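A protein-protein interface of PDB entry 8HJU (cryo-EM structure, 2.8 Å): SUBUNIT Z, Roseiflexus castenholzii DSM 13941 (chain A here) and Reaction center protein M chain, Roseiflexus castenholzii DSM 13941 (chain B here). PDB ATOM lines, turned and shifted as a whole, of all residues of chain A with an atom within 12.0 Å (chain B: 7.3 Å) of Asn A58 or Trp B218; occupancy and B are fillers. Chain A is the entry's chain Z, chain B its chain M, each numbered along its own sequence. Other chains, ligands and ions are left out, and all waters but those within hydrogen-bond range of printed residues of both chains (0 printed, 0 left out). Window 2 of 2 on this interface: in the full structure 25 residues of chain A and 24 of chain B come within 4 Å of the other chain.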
ATOM      1  N   ARG A  51      -7.024   4.737 -24.043  1.00  0.00           N
ATOM      2  CA  ARG A  51      -8.314   4.905 -24.679  1.00  0.00           C
ATOM      3  C   ARG A  51      -8.464   3.843 -25.754  1.00  0.00           C
ATOM      4  O   ARG A  51      -7.483   3.268 -26.221  1.00  0.00           O
ATOM      5  CB  ARG A  51      -8.462   6.298 -25.302  1.00  0.00           C
ATOM      6  CG  ARG A  51      -7.966   7.423 -24.429  1.00  0.00           C
ATOM      7  CD  ARG A  51      -7.549   8.621 -25.250  1.00  0.00           C
ATOM      8  NE  ARG A  51      -6.987   9.681 -24.420  1.00  0.00           N
ATOM      9  CZ  ARG A  51      -7.713  10.475 -23.651  1.00  0.00           C
ATOM     10  NH1 ARG A  51      -9.026  10.327 -23.608  1.00  0.00           N
ATOM     11  NH2 ARG A  51      -7.129  11.411 -22.928  1.00  0.00           N
ATOM     12  N   LEU A  52      -9.702   3.576 -26.136  1.00  0.00           N
ATOM     13  CA  LEU A  52      -9.953   2.773 -27.319  1.00  0.00           C
ATOM     14  C   LEU A  52      -9.726   3.643 -28.540  1.00  0.00           C
ATOM     15  O   LEU A  52     -10.278   4.744 -28.631  1.00  0.00           O
ATOM     16  CB  LEU A  52     -11.377   2.230 -27.316  1.00  0.00           C
ATOM     17  CG  LEU A  52     -11.740   1.306 -26.160  1.00  0.00           C
ATOM     18  CD1 LEU A  52     -13.093   0.686 -26.408  1.00  0.00           C
ATOM     19  CD2 LEU A  52     -10.678   0.242 -25.986  1.00  0.00           C
ATOM     20  N   ASP A  53      -8.911   3.168 -29.473  1.00  0.00           N
ATOM     21  CA  ASP A  53      -8.623   3.976 -30.647  1.00  0.00           C
ATOM     22  C   ASP A  53      -9.922   4.287 -31.386  1.00  0.00           C
ATOM     23  O   ASP A  53     -10.698   3.372 -31.674  1.00  0.00           O
ATOM     24  CB  ASP A  53      -7.641   3.285 -31.588  1.00  0.00           C
ATOM     25  CG  ASP A  53      -7.227   4.181 -32.725  1.00  0.00           C
ATOM     26  OD1 ASP A  53      -6.799   5.322 -32.453  1.00  0.00           O
ATOM     27  OD2 ASP A  53      -7.371   3.775 -33.891  1.00  0.00           O
ATOM     28  N   PRO A  54     -10.181   5.548 -31.726  1.00  0.00           N
ATOM     29  CA  PRO A  54     -11.475   5.867 -32.339  1.00  0.00           C
ATOM     30  C   PRO A  54     -11.640   5.266 -33.719  1.00  0.00           C
ATOM     31  O   PRO A  54     -12.753   4.876 -34.086  1.00  0.00           O
ATOM     32  CB  PRO A  54     -11.471   7.402 -32.380  1.00  0.00           C
ATOM     33  CG  PRO A  54     -10.270   7.833 -31.619  1.00  0.00           C
ATOM     34  CD  PRO A  54      -9.307   6.720 -31.658  1.00  0.00           C
ATOM     35  N   ALA A  55     -10.566   5.189 -34.506  1.00  0.00           N
ATOM     36  CA  ALA A  55     -10.687   4.675 -35.865  1.00  0.00           C
ATOM     37  C   ALA A  55     -11.177   3.233 -35.884  1.00  0.00           C
ATOM     38  O   ALA A  55     -11.870   2.827 -36.822  1.00  0.00           O
ATOM     39  CB  ALA A  55      -9.350   4.788 -36.594  1.00  0.00           C
ATOM     40  N   LYS A  56     -10.841   2.452 -34.859  1.00  0.00           N
ATOM     41  CA  LYS A  56     -11.189   1.037 -34.798  1.00  0.00           C
ATOM     42  C   LYS A  56     -12.516   0.794 -34.094  1.00  0.00           C
ATOM     43  O   LYS A  56     -13.450   0.258 -34.692  1.00  0.00           O
ATOM     44  CB  LYS A  56     -10.093   0.260 -34.066  1.00  0.00           C
ATOM     45  CG  LYS A  56      -8.755   0.248 -34.759  1.00  0.00           C
ATOM     46  CD  LYS A  56      -8.732  -0.766 -35.877  1.00  0.00           C
ATOM     47  CE  LYS A  56      -8.395  -0.111 -37.199  1.00  0.00           C
ATOM     48  NZ  LYS A  56      -7.518  -0.998 -38.007  1.00  0.00           N
ATOM     49  N   ALA A  57     -12.600   1.173 -32.820  1.00  0.00           N
ATOM     50  CA  ALA A  57     -13.769   0.847 -32.010  1.00  0.00           C
ATOM     51  C   ALA A  57     -15.029   1.463 -32.595  1.00  0.00           C
ATOM     52  O   ALA A  57     -16.084   0.819 -32.658  1.00  0.00           O
ATOM     53  CB  ALA A  57     -13.553   1.316 -30.572  1.00  0.00           C
ATOM     54  N   ASN A  58     -14.953   2.723 -32.933  1.00  0.00           N
ATOM     55  CA  ASN A  58     -16.100   3.318 -33.578  1.00  0.00           C
ATOM     56  C   ASN A  58     -16.147   2.725 -34.983  1.00  0.00           C
ATOM     57  O   ASN A  58     -17.207   2.565 -35.573  1.00  0.00           O
ATOM     58  CB  ASN A  58     -16.027   4.855 -33.590  1.00  0.00           C
ATOM     59  CG  ASN A  58     -17.217   5.464 -34.279  1.00  0.00           C
ATOM     60  OD1 ASN A  58     -18.362   5.150 -33.941  1.00  0.00           O
ATOM     61  ND2 ASN A  58     -16.965   6.322 -35.262  1.00  0.00           N
ATOM     62  N   ILE B 212     -24.170  11.175 -20.067  1.00  0.00           N
ATOM     63  CA  ILE B 212     -24.002   9.732 -20.138  1.00  0.00           C
ATOM     64  C   ILE B 212     -25.165   9.091 -20.880  1.00  0.00           C
ATOM     65  O   ILE B 212     -24.991   8.092 -21.583  1.00  0.00           O
ATOM     66  CB  ILE B 212     -23.819   9.152 -18.729  1.00  0.00           C
ATOM     67  CG1 ILE B 212     -22.516   9.662 -18.132  1.00  0.00           C
ATOM     68  CG2 ILE B 212     -23.786   7.659 -18.773  1.00  0.00           C
ATOM     69  CD1 ILE B 212     -21.333   9.499 -19.025  1.00  0.00           C
ATOM     70  N   VAL B 213     -26.364   9.656 -20.759  1.00  0.00           N
ATOM     71  CA  VAL B 213     -27.477   9.130 -21.535  1.00  0.00           C
ATOM     72  C   VAL B 213     -27.332   9.510 -23.003  1.00  0.00           C
ATOM     73  O   VAL B 213     -27.799   8.784 -23.886  1.00  0.00           O
ATOM     74  CB  VAL B 213     -28.814   9.609 -20.941  1.00  0.00           C
ATOM     75  CG1 VAL B 213     -29.973   9.138 -21.777  1.00  0.00           C
ATOM     76  CG2 VAL B 213     -28.971   9.094 -19.536  1.00  0.00           C
ATOM     77  N   ALA B 214     -26.679  10.635 -23.298  1.00  0.00           N
ATOM     78  CA  ALA B 214     -26.473  11.020 -24.687  1.00  0.00           C
ATOM     79  C   ALA B 214     -25.418  10.150 -25.348  1.00  0.00           C
ATOM     80  O   ALA B 214     -25.577   9.736 -26.501  1.00  0.00           O
ATOM     81  CB  ALA B 214     -26.076  12.489 -24.768  1.00  0.00           C
ATOM     82  N   THR B 215     -24.332   9.863 -24.638  1.00  0.00           N
ATOM     83  CA  THR B 215     -23.311   8.948 -25.126  1.00  0.00           C
ATOM     84  C   THR B 215     -23.584   7.512 -24.710  1.00  0.00           C
ATOM     85  O   THR B 215     -22.654   6.708 -24.604  1.00  0.00           O
ATOM     86  CB  THR B 215     -21.936   9.400 -24.644  1.00  0.00           C
ATOM     87  OG1 THR B 215     -21.944   9.511 -23.218  1.00  0.00           O
ATOM     88  CG2 THR B 215     -21.599  10.746 -25.232  1.00  0.00           C
ATOM     89  N   SER B 216     -24.851   7.175 -24.477  1.00  0.00           N
ATOM     90  CA  SER B 216     -25.208   5.857 -23.972  1.00  0.00           C
ATOM     91  C   SER B 216     -25.042   4.778 -25.030  1.00  0.00           C
ATOM     92  O   SER B 216     -24.815   3.613 -24.691  1.00  0.00           O
ATOM     93  CB  SER B 216     -26.645   5.881 -23.465  1.00  0.00           C
ATOM     94  OG  SER B 216     -26.830   4.939 -22.437  1.00  0.00           O
ATOM     95  N   LYS B 217     -25.159   5.140 -26.308  1.00  0.00           N
ATOM     96  CA  LYS B 217     -25.055   4.152 -27.375  1.00  0.00           C
ATOM     97  C   LYS B 217     -23.700   3.468 -27.382  1.00  0.00           C
ATOM     98  O   LYS B 217     -23.594   2.298 -27.766  1.00  0.00           O
ATOM     99  CB  LYS B 217     -25.315   4.818 -28.722  1.00  0.00           C
ATOM    100  CG  LYS B 217     -25.334   3.862 -29.883  1.00  0.00           C
ATOM    101  CD  LYS B 217     -24.755   4.501 -31.120  1.00  0.00           C
ATOM    102  CE  LYS B 217     -25.814   5.262 -31.868  1.00  0.00           C
ATOM    103  NZ  LYS B 217     -25.291   5.794 -33.148  1.00  0.00           N
ATOM    104  N   TRP B 218     -22.655   4.174 -26.965  1.00  0.00           N
ATOM    105  CA  TRP B 218     -21.310   3.632 -26.923  1.00  0.00           C
ATOM    106  C   TRP B 218     -20.911   3.194 -25.525  1.00  0.00           C
ATOM    107  O   TRP B 218     -19.719   3.134 -25.217  1.00  0.00           O
ATOM    108  CB  TRP B 218     -20.326   4.655 -27.479  1.00  0.00           C
ATOM    109  CG  TRP B 218     -20.739   5.167 -28.811  1.00  0.00           C
ATOM    110  CD1 TRP B 218     -20.497   4.589 -30.013  1.00  0.00           C
ATOM    111  CD2 TRP B 218     -21.485   6.357 -29.080  1.00  0.00           C
ATOM    112  NE1 TRP B 218     -21.039   5.342 -31.019  1.00  0.00           N
ATOM    113  CE2 TRP B 218     -21.652   6.436 -30.470  1.00  0.00           C
ATOM    114  CE3 TRP B 218     -22.029   7.363 -28.280  1.00  0.00           C
ATOM    115  CZ2 TRP B 218     -22.335   7.479 -31.078  1.00  0.00           C
ATOM    116  CZ3 TRP B 218     -22.703   8.395 -28.884  1.00  0.00           C
ATOM    117  CH2 TRP B 218     -22.852   8.447 -30.268  1.00  0.00           C
ATOM    118  N   LYS B 219     -21.892   2.901 -24.674  1.00  0.00           N
ATOM    119  CA  LYS B 219     -21.665   2.304 -23.358  1.00  0.00           C
ATOM    120  C   LYS B 219     -20.794   3.187 -22.475  1.00  0.00           C
ATOM    121  O   LYS B 219     -19.864   2.718 -21.820  1.00  0.00           O
ATOM    122  CB  LYS B 219     -21.069   0.905 -23.484  1.00  0.00           C
ATOM    123  CG  LYS B 219     -22.047  -0.112 -24.025  1.00  0.00           C
ATOM    124  CD  LYS B 219     -23.420   0.098 -23.418  1.00  0.00           C
ATOM    125  CE  LYS B 219     -24.513  -0.451 -24.311  1.00  0.00           C
ATOM    126  NZ  LYS B 219     -25.840   0.149 -23.994  1.00  0.00           N
ATOM    127  N   SER B 220     -21.103   4.483 -22.455  1.00  0.00           N
ATOM    128  CA  SER B 220     -20.416   5.395 -21.555  1.00  0.00           C
ATOM    129  C   SER B 220     -20.807   5.172 -20.103  1.00  0.00           C
ATOM    130  O   SER B 220     -20.067   5.585 -19.207  1.00  0.00           O
ATOM    131  CB  SER B 220     -20.716   6.836 -21.946  1.00  0.00           C
ATOM    132  OG  SER B 220     -22.059   7.160 -21.647  1.00  0.00           O
ATOM    133  N   GLU B 221     -21.953   4.533 -19.855  1.00  0.00           N
ATOM    134  CA  GLU B 221     -22.459   4.403 -18.494  1.00  0.00           C
ATOM    135  C   GLU B 221     -21.653   3.407 -17.678  1.00  0.00           C
ATOM    136  O   GLU B 221     -21.671   3.464 -16.446  1.00  0.00           O
ATOM    137  CB  GLU B 221     -23.927   3.988 -18.521  1.00  0.00           C
ATOM    138  CG  GLU B 221     -24.169   2.614 -19.119  1.00  0.00           C
ATOM    139  CD  GLU B 221     -24.408   2.661 -20.608  1.00  0.00           C
ATOM    140  OE1 GLU B 221     -25.207   1.848 -21.112  1.00  0.00           O
ATOM    141  OE2 GLU B 221     -23.803   3.516 -21.279  1.00  0.00           O
ATOM    142  N   MET B 222     -20.955   2.486 -18.336  1.00  0.00           N
ATOM    143  CA  MET B 222     -20.150   1.489 -17.639  1.00  0.00           C
ATOM    144  C   MET B 222     -18.868   2.164 -17.171  1.00  0.00           C
ATOM    145  O   MET B 222     -17.790   1.988 -17.738  1.00  0.00           O
ATOM    146  CB  MET B 222     -19.867   0.297 -18.540  1.00  0.00           C
ATOM    147  CG  MET B 222     -21.067  -0.166 -19.330  1.00  0.00           C
ATOM    148  SD  MET B 222     -22.443  -0.640 -18.275  1.00  0.00           S
ATOM    149  CE  MET B 222     -21.733  -2.031 -17.404  1.00  0.00           C
ATOM    150  N   GLU B 226     -14.929   2.110 -18.226  1.00  0.00           N
ATOM    151  CA  GLU B 226     -14.400   3.318 -18.848  1.00  0.00           C
ATOM    152  C   GLU B 226     -13.221   3.883 -18.073  1.00  0.00           C
ATOM    153  O   GLU B 226     -12.398   4.604 -18.642  1.00  0.00           O
ATOM    154  CB  GLU B 226     -15.500   4.367 -18.972  1.00  0.00           C
ATOM    155  CG  GLU B 226     -16.652   3.957 -19.849  1.00  0.00           C
ATOM    156  CD  GLU B 226     -16.222   3.607 -21.254  1.00  0.00           C
ATOM    157  OE1 GLU B 226     -15.964   4.534 -22.046  1.00  0.00           O
ATOM    158  OE2 GLU B 226     -16.147   2.404 -21.572  1.00  0.00           O
ATOM    159  N   GLY B 231     -13.711   4.489 -23.712  1.00  0.00           N
ATOM    160  CA  GLY B 231     -14.262   4.112 -24.989  1.00  0.00           C
ATOM    161  C   GLY B 231     -14.739   5.306 -25.780  1.00  0.00           C
ATOM    162  O   GLY B 231     -14.555   6.464 -25.401  1.00  0.00           O
ATOM    163  N   PRO B 232     -15.374   5.022 -26.920  1.00  0.00           N
ATOM    164  CA  PRO B 232     -15.812   6.115 -27.801  1.00  0.00           C
ATOM    165  C   PRO B 232     -16.890   6.997 -27.198  1.00  0.00           C
ATOM    166  O   PRO B 232     -16.937   8.191 -27.512  1.00  0.00           O
ATOM    167  CB  PRO B 232     -16.314   5.378 -29.048  1.00  0.00           C
ATOM    168  CG  PRO B 232     -16.599   4.007 -28.592  1.00  0.00           C
ATOM    169  CD  PRO B 232     -15.622   3.702 -27.513  1.00  0.00           C
ATOM    170  N   GLY B 233     -17.756   6.457 -26.341  1.00  0.00           N
ATOM    171  CA  GLY B 233     -18.769   7.289 -25.714  1.00  0.00           C
ATOM    172  C   GLY B 233     -18.181   8.300 -24.751  1.00  0.00           C
ATOM    173  O   GLY B 233     -18.560   9.472 -24.759  1.00  0.00           O
ATOM    174  N   THR B 234     -17.245   7.864 -23.910  1.00  0.00           N
ATOM    175  CA  THR B 234     -16.572   8.796 -23.016  1.00  0.00           C
ATOM    176  C   THR B 234     -15.753   9.813 -23.796  1.00  0.00           C
ATOM    177  O   THR B 234     -15.653  10.978 -23.399  1.00  0.00           O
ATOM    178  CB  THR B 234     -15.682   8.036 -22.040  1.00  0.00           C
ATOM    179  OG1 THR B 234     -16.448   7.012 -21.402  1.00  0.00           O
ATOM    180  CG2 THR B 234     -15.142   8.974 -20.991  1.00  0.00           C
ATOM    181  N   GLN B 235     -15.156   9.391 -24.909  1.00  0.00           N
ATOM    182  CA  GLN B 235     -14.441  10.332 -25.760  1.00  0.00           C
ATOM    183  C   GLN B 235     -15.378  11.400 -26.297  1.00  0.00           C
ATOM    184  O   GLN B 235     -15.049  12.592 -26.284  1.00  0.00           O
ATOM    185  CB  GLN B 235     -13.762   9.586 -26.904  1.00  0.00           C
ATOM    186  CG  GLN B 235     -12.574   8.764 -26.470  1.00  0.00           C
ATOM    187  CD  GLN B 235     -12.263   7.639 -27.422  1.00  0.00           C
ATOM    188  OE1 GLN B 235     -12.662   7.668 -28.581  1.00  0.00           O
ATOM    189  NE2 GLN B 235     -11.550   6.638 -26.938  1.00  0.00           N
ATOM    190  N   ARG B 236     -16.555  10.995 -26.770  1.00  0.00           N
ATOM    191  CA  ARG B 236     -17.519  11.968 -27.265  1.00  0.00           C
ATOM    192  C   ARG B 236     -18.000  12.885 -26.150  1.00  0.00           C
ATOM    193  O   ARG B 236     -18.250  14.066 -26.384  1.00  0.00           O
ATOM    194  CB  ARG B 236     -18.697  11.255 -27.916  1.00  0.00           C
ATOM    195  CG  ARG B 236     -18.460  10.900 -29.352  1.00  0.00           C
ATOM    196  CD  ARG B 236     -19.508   9.949 -29.844  1.00  0.00           C
ATOM    197  NE  ARG B 236     -18.919   8.816 -30.541  1.00  0.00           N
ATOM    198  CZ  ARG B 236     -18.993   8.633 -31.850  1.00  0.00           C
ATOM    199  NH1 ARG B 236     -19.630   9.513 -32.603  1.00  0.00           N
ATOM    200  NH2 ARG B 236     -18.432   7.572 -32.405  1.00  0.00           N
ATOM    201  N   ALA B 237     -18.134  12.361 -24.935  1.00  0.00           N
ATOM    202  CA  ALA B 237     -18.548  13.191 -23.809  1.00  0.00           C
ATOM    203  C   ALA B 237     -17.502  14.255 -23.493  1.00  0.00           C
ATOM    204  O   ALA B 237     -17.824  15.443 -23.322  1.00  0.00           O
ATOM    205  CB  ALA B 237     -18.802  12.307 -22.594  1.00  0.00           C
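The side-chain amide nitrogen (NE2) of Gln B235 sits at hydrogen-bond distance from the backbone carbonyl oxygen (O) of Leu A52, at 2.8 Å. The side-chain amide oxygen (OD1) of Asn A58 sits at hydrogen-bond distance from the guanidinium group (NH2) of Arg B236 (2.9 Å).
OE1 of Glu B226 is in hydrogen-bond range of N of Gly B231 (2.8 Å). The backbone carbonyl oxygen (O) of Gly B231 lies close to the side-chain amide nitrogen (NE2) of Gln B235, 3.4 Å away.
Among the printed residues, pairs that only touch across the chains: Arg A51 with Gln B235 (3.5 Å), Leu A52 with Gly B231 (3.9 Å), Pro A54 with Gln B235 (3.9 Å) and Asn A58 with Trp B218 (3.97 Å).
Asn A58 touches just these residues of chain B: Trp B218 (3.97 Å) and Arg B236 (2.9 Å). Trp B218 touches just one residue of chain A: Asn A58 (3.97 Å). No residue of chain B comes within 4 Å of Ala A57. No residue of chain A comes within 4 Å of Ala B214. No residue of chain A comes within 4 Å of Thr B215. No residue of chain A comes within 4 Å of Ser B216. Lys B219 touches none of the printed residues of chain A. Pro B232 touches none of the printed residues of chain A. Arg B236 touches one residue of chain A. Of the printed residues of chain A, Gln B235 touches Arg A51 (3.5 Å), Leu A52 (2.8 Å) and Pro A54 (3.9 Å). Of the printed residues of chain B, Pro A54 touches Gln B235. Glu B226 touches none of the printed residues of chain A. The nearest residue of chain A that does not touch Trp B218 is Ala A57 (6.4 Å).
Hydrophobic or aromatic side chains of chain A that line the printed part of chain B: Leu A52 and Pro A54. Among the printed residues, 6 pairs touch across the chains.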
